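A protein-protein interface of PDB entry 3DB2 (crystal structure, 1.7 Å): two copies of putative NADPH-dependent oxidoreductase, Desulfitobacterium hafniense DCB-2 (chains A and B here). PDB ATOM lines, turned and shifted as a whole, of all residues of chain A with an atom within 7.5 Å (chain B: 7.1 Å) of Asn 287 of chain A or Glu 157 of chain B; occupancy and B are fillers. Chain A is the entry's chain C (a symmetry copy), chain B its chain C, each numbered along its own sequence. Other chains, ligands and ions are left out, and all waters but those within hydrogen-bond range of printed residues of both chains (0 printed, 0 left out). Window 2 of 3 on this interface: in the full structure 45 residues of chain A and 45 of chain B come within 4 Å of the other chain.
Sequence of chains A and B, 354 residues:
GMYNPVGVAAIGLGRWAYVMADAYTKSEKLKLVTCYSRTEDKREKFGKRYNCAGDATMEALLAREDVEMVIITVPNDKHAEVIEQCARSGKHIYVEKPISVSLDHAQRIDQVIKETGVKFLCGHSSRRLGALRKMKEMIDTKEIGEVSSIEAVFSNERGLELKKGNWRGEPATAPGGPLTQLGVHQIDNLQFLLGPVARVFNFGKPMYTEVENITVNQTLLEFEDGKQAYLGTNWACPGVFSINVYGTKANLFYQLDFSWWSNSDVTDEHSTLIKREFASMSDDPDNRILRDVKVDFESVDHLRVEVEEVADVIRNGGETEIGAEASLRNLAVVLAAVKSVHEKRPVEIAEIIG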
ATOM      1  N   GLY A 247     -29.196   9.309 -10.214  1.00  0.00           N
ATOM      2  CA  GLY A 247     -30.512   9.790 -10.600  1.00  0.00           C
ATOM      3  C   GLY A 247     -30.446  10.486 -11.942  1.00  0.00           C
ATOM      4  O   GLY A 247     -29.329  10.842 -12.365  1.00  0.00           O
ATOM      5  N   THR A 248     -31.614  10.619 -12.608  1.00  0.00           N
ATOM      6  CA  THR A 248     -31.570  11.180 -13.975  1.00  0.00           C
ATOM      7  C   THR A 248     -31.334  12.679 -13.950  1.00  0.00           C
ATOM      8  O   THR A 248     -30.882  13.236 -14.959  1.00  0.00           O
ATOM      9  CB  THR A 248     -32.854  10.847 -14.768  1.00  0.00           C
ATOM     10  OG1 THR A 248     -33.954  11.266 -13.937  1.00  0.00           O
ATOM     11  CG2 THR A 248     -33.033   9.353 -15.019  1.00  0.00           C
ATOM     12  N   GLU A 277     -25.299  17.870  -9.503  1.00  0.00           N
ATOM     13  CA  GLU A 277     -26.451  18.177 -10.350  1.00  0.00           C
ATOM     14  C   GLU A 277     -26.026  19.075 -11.496  1.00  0.00           C
ATOM     15  O   GLU A 277     -24.936  19.632 -11.401  1.00  0.00           O
ATOM     16  CB  GLU A 277     -27.541  18.888  -9.534  1.00  0.00           C
ATOM     17  CG  GLU A 277     -27.001  20.196  -8.987  1.00  0.00           C
ATOM     18  CD  GLU A 277     -27.969  21.014  -8.181  1.00  0.00           C
ATOM     19  OE1 GLU A 277     -29.138  20.606  -8.099  1.00  0.00           O
ATOM     20  OE2 GLU A 277     -27.517  22.044  -7.636  1.00  0.00           O
ATOM     21  N   PHE A 278     -26.858  19.201 -12.518  1.00  0.00           N
ATOM     22  CA  PHE A 278     -26.562  20.121 -13.609  1.00  0.00           C
ATOM     23  C   PHE A 278     -26.769  21.535 -13.069  1.00  0.00           C
ATOM     24  O   PHE A 278     -27.769  21.736 -12.386  1.00  0.00           O
ATOM     25  CB  PHE A 278     -27.429  19.879 -14.838  1.00  0.00           C
ATOM     26  CG  PHE A 278     -27.385  18.455 -15.353  1.00  0.00           C
ATOM     27  CD1 PHE A 278     -26.279  18.036 -16.083  1.00  0.00           C
ATOM     28  CD2 PHE A 278     -28.415  17.577 -15.092  1.00  0.00           C
ATOM     29  CE1 PHE A 278     -26.224  16.738 -16.554  1.00  0.00           C
ATOM     30  CE2 PHE A 278     -28.374  16.280 -15.574  1.00  0.00           C
ATOM     31  CZ  PHE A 278     -27.266  15.870 -16.299  1.00  0.00           C
ATOM     32  N   ALA A 279     -25.828  22.398 -13.391  1.00  0.00           N
ATOM     33  CA  ALA A 279     -25.855  23.820 -13.058  1.00  0.00           C
ATOM     34  C   ALA A 279     -26.030  24.618 -14.355  1.00  0.00           C
ATOM     35  O   ALA A 279     -26.282  24.034 -15.417  1.00  0.00           O
ATOM     36  CB  ALA A 279     -24.604  24.239 -12.304  1.00  0.00           C
ATOM     37  N   ASN A 287     -28.372  19.917 -18.634  1.00  0.00           N
ATOM     38  CA  ASN A 287     -27.351  20.948 -18.793  1.00  0.00           C
ATOM     39  C   ASN A 287     -25.994  20.339 -19.156  1.00  0.00           C
ATOM     40  O   ASN A 287     -25.882  19.125 -19.326  1.00  0.00           O
ATOM     41  CB  ASN A 287     -27.208  21.799 -17.529  1.00  0.00           C
ATOM     42  N   ARG A 288     -25.003  21.222 -19.265  1.00  0.00           N
ATOM     43  CA  ARG A 288     -23.663  20.894 -19.730  1.00  0.00           C
ATOM     44  C   ARG A 288     -22.566  21.318 -18.757  1.00  0.00           C
ATOM     45  O   ARG A 288     -21.373  21.224 -19.072  1.00  0.00           O
ATOM     46  CB  ARG A 288     -23.419  21.548 -21.095  1.00  0.00           C
ATOM     47  N   ILE A 289     -22.948  21.776 -17.576  1.00  0.00           N
ATOM     48  CA  ILE A 289     -22.030  21.992 -16.470  1.00  0.00           C
ATOM     49  C   ILE A 289     -22.620  21.347 -15.207  1.00  0.00           C
ATOM     50  O   ILE A 289     -23.836  21.410 -15.024  1.00  0.00           O
ATOM     51  CB  ILE A 289     -21.768  23.457 -16.108  1.00  0.00           C
ATOM     52  CG1 ILE A 289     -20.779  23.674 -14.963  1.00  0.00           C
ATOM     53  CG2 ILE A 289     -23.098  24.125 -15.785  1.00  0.00           C
ATOM     54  CD1 ILE A 289     -19.335  23.517 -15.372  1.00  0.00           C
ATOM     55  N   LEU A 290     -21.744  20.784 -14.394  1.00  0.00           N
ATOM     56  CA  LEU A 290     -22.154  20.136 -13.149  1.00  0.00           C
ATOM     57  C   LEU A 290     -21.602  20.839 -11.913  1.00  0.00           C
ATOM     58  O   LEU A 290     -20.476  21.357 -11.891  1.00  0.00           O
ATOM     59  CB  LEU A 290     -21.686  18.683 -13.193  1.00  0.00           C
ATOM     60  CG  LEU A 290     -22.318  17.752 -14.221  1.00  0.00           C
ATOM     61  CD1 LEU A 290     -21.577  16.419 -14.250  1.00  0.00           C
ATOM     62  CD2 LEU A 290     -23.791  17.548 -13.921  1.00  0.00           C
ATOM     63  N   SER B 155     -20.012   7.127 -16.109  1.00  0.00           N
ATOM     64  CA  SER B 155     -21.383   7.453 -16.448  1.00  0.00           C
ATOM     65  C   SER B 155     -21.520   8.878 -16.992  1.00  0.00           C
ATOM     66  O   SER B 155     -20.705   9.776 -16.742  1.00  0.00           O
ATOM     67  CB  SER B 155     -22.308   7.342 -15.241  1.00  0.00           C
ATOM     68  OG  SER B 155     -22.082   8.411 -14.335  1.00  0.00           O
ATOM     69  N   ASN B 156     -22.601   9.066 -17.724  1.00  0.00           N
ATOM     70  CA  ASN B 156     -23.045  10.381 -18.198  1.00  0.00           C
ATOM     71  C   ASN B 156     -24.501  10.239 -18.635  1.00  0.00           C
ATOM     72  O   ASN B 156     -25.115   9.168 -18.558  1.00  0.00           O
ATOM     73  CB  ASN B 156     -22.103  10.906 -19.259  1.00  0.00           C
ATOM     74  CG  ASN B 156     -22.171  10.174 -20.576  1.00  0.00           C
ATOM     75  OD1 ASN B 156     -23.159   9.590 -20.998  1.00  0.00           O
ATOM     76  ND2 ASN B 156     -21.020  10.248 -21.224  1.00  0.00           N
ATOM     77  N   GLU B 157     -25.091  11.344 -19.072  1.00  0.00           N
ATOM     78  CA  GLU B 157     -26.537  11.362 -19.288  1.00  0.00           C
ATOM     79  C   GLU B 157     -26.880  11.110 -20.741  1.00  0.00           C
ATOM     80  O   GLU B 157     -28.009  11.404 -21.174  1.00  0.00           O
ATOM     81  CB  GLU B 157     -26.991  12.735 -18.779  1.00  0.00           C
ATOM     82  CG  GLU B 157     -26.594  13.805 -19.762  1.00  0.00           C
ATOM     83  CD  GLU B 157     -25.254  14.475 -19.548  1.00  0.00           C
ATOM     84  OE1 GLU B 157     -24.332  13.896 -18.934  1.00  0.00           O
ATOM     85  OE2 GLU B 157     -25.136  15.633 -20.029  1.00  0.00           O
ATOM     86  N   ARG B 158     -25.956  10.532 -21.506  1.00  0.00           N
ATOM     87  CA  ARG B 158     -26.198  10.350 -22.942  1.00  0.00           C
ATOM     88  C   ARG B 158     -27.510   9.664 -23.305  1.00  0.00           C
ATOM     89  O   ARG B 158     -28.201  10.037 -24.280  1.00  0.00           O
ATOM     90  CB  ARG B 158     -25.039   9.545 -23.554  1.00  0.00           C
ATOM     91  CG  ARG B 158     -25.344   9.114 -24.980  1.00  0.00           C
ATOM     92  CD  ARG B 158     -24.698  10.081 -25.952  1.00  0.00           C
ATOM     93  NE  ARG B 158     -23.275  10.248 -25.725  1.00  0.00           N
ATOM     94  CZ  ARG B 158     -22.554  11.282 -26.137  1.00  0.00           C
ATOM     95  NH1 ARG B 158     -23.098  12.281 -26.821  1.00  0.00           N
ATOM     96  NH2 ARG B 158     -21.263  11.323 -25.868  1.00  0.00           N
ATOM     97  N   GLY B 159     -27.885   8.639 -22.539  1.00  0.00           N
ATOM     98  CA  GLY B 159     -29.048   7.826 -22.866  1.00  0.00           C
ATOM     99  C   GLY B 159     -30.374   8.566 -22.787  1.00  0.00           C
ATOM    100  O   GLY B 159     -31.351   8.211 -23.449  1.00  0.00           O
ATOM    101  N   LEU B 160     -30.412   9.596 -21.972  1.00  0.00           N
ATOM    102  CA  LEU B 160     -31.599  10.347 -21.610  1.00  0.00           C
ATOM    103  C   LEU B 160     -32.088  11.149 -22.832  1.00  0.00           C
ATOM    104  O   LEU B 160     -33.285  11.410 -22.903  1.00  0.00           O
ATOM    105  CB  LEU B 160     -31.314  11.278 -20.443  1.00  0.00           C
ATOM    106  CG  LEU B 160     -30.919  10.655 -19.100  1.00  0.00           C
ATOM    107  CD1 LEU B 160     -30.833  11.721 -18.016  1.00  0.00           C
ATOM    108  CD2 LEU B 160     -31.900   9.554 -18.724  1.00  0.00           C
ATOM    109  N   GLU B 161     -31.142  11.497 -23.686  1.00  0.00           N
ATOM    110  CA  GLU B 161     -31.411  12.368 -24.832  1.00  0.00           C
ATOM    111  C   GLU B 161     -31.416  11.603 -26.153  1.00  0.00           C
ATOM    112  O   GLU B 161     -31.972  12.091 -27.144  1.00  0.00           O
ATOM    113  CB  GLU B 161     -30.365  13.483 -24.920  1.00  0.00           C
ATOM    114  CG  GLU B 161     -29.818  13.672 -26.322  1.00  0.00           C
ATOM    115  CD  GLU B 161     -29.843  15.097 -26.837  1.00  0.00           C
ATOM    116  OE1 GLU B 161     -29.928  16.042 -26.020  1.00  0.00           O
ATOM    117  OE2 GLU B 161     -29.779  15.297 -28.073  1.00  0.00           O
ATOM    118  N   LEU B 162     -30.803  10.433 -26.141  1.00  0.00           N
ATOM    119  CA  LEU B 162     -30.717   9.555 -27.302  1.00  0.00           C
ATOM    120  C   LEU B 162     -32.101   9.298 -27.897  1.00  0.00           C
ATOM    121  O   LEU B 162     -32.884   8.501 -27.388  1.00  0.00           O
ATOM    122  CB  LEU B 162     -30.084   8.204 -26.968  1.00  0.00           C
ATOM    123  CG  LEU B 162     -28.598   7.907 -26.975  1.00  0.00           C
ATOM    124  CD1 LEU B 162     -28.356   6.416 -26.718  1.00  0.00           C
ATOM    125  CD2 LEU B 162     -27.884   8.290 -28.263  1.00  0.00           C
ATOM    126  N   LEU B 182     -18.001   3.828 -22.747  1.00  0.00           N
ATOM    127  CA  LEU B 182     -17.469   4.310 -21.479  1.00  0.00           C
ATOM    128  C   LEU B 182     -16.682   3.179 -20.827  1.00  0.00           C
ATOM    129  O   LEU B 182     -15.554   3.375 -20.377  1.00  0.00           O
ATOM    130  CB  LEU B 182     -18.568   4.797 -20.527  1.00  0.00           C
ATOM    131  CG  LEU B 182     -19.520   5.880 -21.032  1.00  0.00           C
ATOM    132  CD1 LEU B 182     -20.418   6.409 -19.908  1.00  0.00           C
ATOM    133  CD2 LEU B 182     -18.739   7.017 -21.665  1.00  0.00           C
ATOM    134  N   ASN B 234     -23.294   3.790 -16.958  1.00  0.00           N
ATOM    135  CA  ASN B 234     -24.650   4.297 -16.838  1.00  0.00           C
ATOM    136  C   ASN B 234     -24.825   5.460 -17.804  1.00  0.00           C
ATOM    137  O   ASN B 234     -23.933   6.318 -17.810  1.00  0.00           O
ATOM    138  CB  ASN B 234     -24.791   4.661 -15.352  1.00  0.00           C
ATOM    139  CG  ASN B 234     -26.220   4.951 -14.955  1.00  0.00           C
ATOM    140  OD1 ASN B 234     -26.854   5.654 -15.733  1.00  0.00           O
ATOM    141  ND2 ASN B 234     -26.659   4.433 -13.801  1.00  0.00           N
ATOM    142  N   TRP B 235     -25.895   5.457 -18.579  1.00  0.00           N
ATOM    143  CA  TRP B 235     -26.133   6.534 -19.555  1.00  0.00           C
ATOM    144  C   TRP B 235     -27.329   7.372 -19.142  1.00  0.00           C
ATOM    145  O   TRP B 235     -27.937   8.044 -19.960  1.00  0.00           O
ATOM    146  CB  TRP B 235     -26.304   5.958 -20.973  1.00  0.00           C
ATOM    147  CG  TRP B 235     -25.103   6.067 -21.865  1.00  0.00           C
ATOM    148  CD1 TRP B 235     -23.956   6.798 -21.681  1.00  0.00           C
ATOM    149  CD2 TRP B 235     -24.918   5.404 -23.133  1.00  0.00           C
ATOM    150  NE1 TRP B 235     -23.103   6.632 -22.709  1.00  0.00           N
ATOM    151  CE2 TRP B 235     -23.657   5.780 -23.636  1.00  0.00           C
ATOM    152  CE3 TRP B 235     -25.672   4.529 -23.921  1.00  0.00           C
ATOM    153  CZ2 TRP B 235     -23.123   5.340 -24.845  1.00  0.00           C
ATOM    154  CZ3 TRP B 235     -25.135   4.096 -25.118  1.00  0.00           C
ATOM    155  CH2 TRP B 235     -23.881   4.484 -25.589  1.00  0.00           C
ATOM    156  N   ALA B 236     -27.684   7.290 -17.863  1.00  0.00           N
ATOM    157  CA  ALA B 236     -28.927   7.846 -17.335  1.00  0.00           C
ATOM    158  C   ALA B 236     -28.731   8.763 -16.147  1.00  0.00           C
ATOM    159  O   ALA B 236     -29.680   8.903 -15.362  1.00  0.00           O
ATOM    160  CB  ALA B 236     -29.822   6.659 -16.955  1.00  0.00           C
ATOM    161  N   CYS B 237     -27.524   9.342 -16.006  1.00  0.00           N
ATOM    162  CA  CYS B 237     -27.258  10.247 -14.899  1.00  0.00           C
ATOM    163  C   CYS B 237     -26.133  11.232 -15.161  1.00  0.00           C
ATOM    164  O   CYS B 237     -25.347  11.117 -16.090  1.00  0.00           O
ATOM    165  CB  CYS B 237     -26.952   9.410 -13.630  1.00  0.00           C
ATOM    166  SG  CYS B 237     -25.462   8.383 -13.842  1.00  0.00           S
ATOM    167  N   PRO B 238     -26.012  12.279 -14.350  1.00  0.00           N
ATOM    168  CA  PRO B 238     -24.878  13.189 -14.522  1.00  0.00           C
ATOM    169  C   PRO B 238     -23.520  12.490 -14.482  1.00  0.00           C
ATOM    170  O   PRO B 238     -23.382  11.423 -13.867  1.00  0.00           O
ATOM    171  CB  PRO B 238     -25.008  14.135 -13.345  1.00  0.00           C
ATOM    172  CG  PRO B 238     -26.488  14.165 -13.100  1.00  0.00           C
ATOM    173  CD  PRO B 238     -26.924  12.722 -13.277  1.00  0.00           C
ATOM    174  N   GLY B 239     -22.541  13.092 -15.162  1.00  0.00           N
ATOM    175  CA  GLY B 239     -21.247  12.484 -15.381  1.00  0.00           C
ATOM    176  C   GLY B 239     -20.472  12.160 -14.109  1.00  0.00           C
ATOM    177  O   GLY B 239     -20.337  12.973 -13.188  1.00  0.00           O
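The backbone NH of Ala 236 of chain B sits at hydrogen-bond distance from the side-chain amide oxygen of Asn 234 of chain B (2.8 Å). The backbone NH of Ala 236 of chain B is in hydrogen-bond range of the backbone carbonyl oxygen of Asn 156 of chain B (3.3 Å). O of Cys 237 of chain B is in hydrogen-bond range of N of Glu 157 of chain B (3.0 Å). The side-chain amide oxygen (OD1) of Asn 234 of chain B is in hydrogen-bond range of the side-chain sulfur (SG) of Cys 237 of chain B (3.6 Å). The side-chain sulfur of Cys 237 of chain B sits at hydrogen-bond distance from the side-chain hydroxyl of Ser 155 of chain B, 3.4 Å away. O of Pro 238 of chain B sits at hydrogen-bond distance from OG of Ser 155 of chain B (3.3 Å).
Asn 287 of chain A touches one residue of chain B. Glu 157 of chain B touches two residues of chain A. Of the printed residues of chain A, Ala 236 of chain B touches Gly 247 and Thr 248. Of the printed residues of chain A, Leu 160 of chain B touches Thr 248 (3.4 Å). Of the printed residues of chain A, Cys 237 of chain B touches Gly 247. Of the printed residues of chain B, Gly 247 of chain A touches Ala 236, Cys 237 and Pro 238. Leu 162 of chain B touches none of the printed residues of chain A. Ser 155 of chain B touches none of the printed residues of chain A. The nearest printed residue of chain A that does not touch Glu 157 of chain B is Arg 288 of chain A (5.5 Å).
Hydrophobic or aromatic side chains of chain B within 4 Å of the printed part of chain A: Leu 160 and Pro 238. Printed residues of chain A that touch a printed residue of chain B: Gly 247, Thr 248, Phe 278, Asn 287 and Leu 290. Hydrophobic or aromatic side chains of chain A that line the printed part of chain B: Phe 278 and Leu 290. Along chain A the printed residues that touch a printed residue of chain B span positions 247 to 290. Among the printed residues, 10 pairs touch across the chains. Among the printed residues, no Asp or Glu carboxylate lies within 4 Å of a Lys or Arg side-chain nitrogen of the other chain.
O of Ala 236 of chain B touches O of Gly 247 of chain A, 3.6 Å away. Cys 237 of chain B touches Gly 247 of chain A (CB to O, 3.0 Å). Gly 247 of chain A touches Pro 238 of chain B (O to CD, 3.2 Å). Thr 248 of chain A touches Leu 160 of chain B. Ala 236 of chain B touches Thr 248 of chain A. Phe 278 of chain A touches Glu 157 of chain B. CG of Pro 238 of chain B touches CZ of Phe 278 of chain A (3.7 Å). Glu 157 of chain B touches Asn 287 of chain A. Leu 290 of chain A touches Pro 238 of chain B (CD2 to CB, 3.7 Å). Gly 239 of chain B touches Leu 290 of chain A.
No position is printed for both chains.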
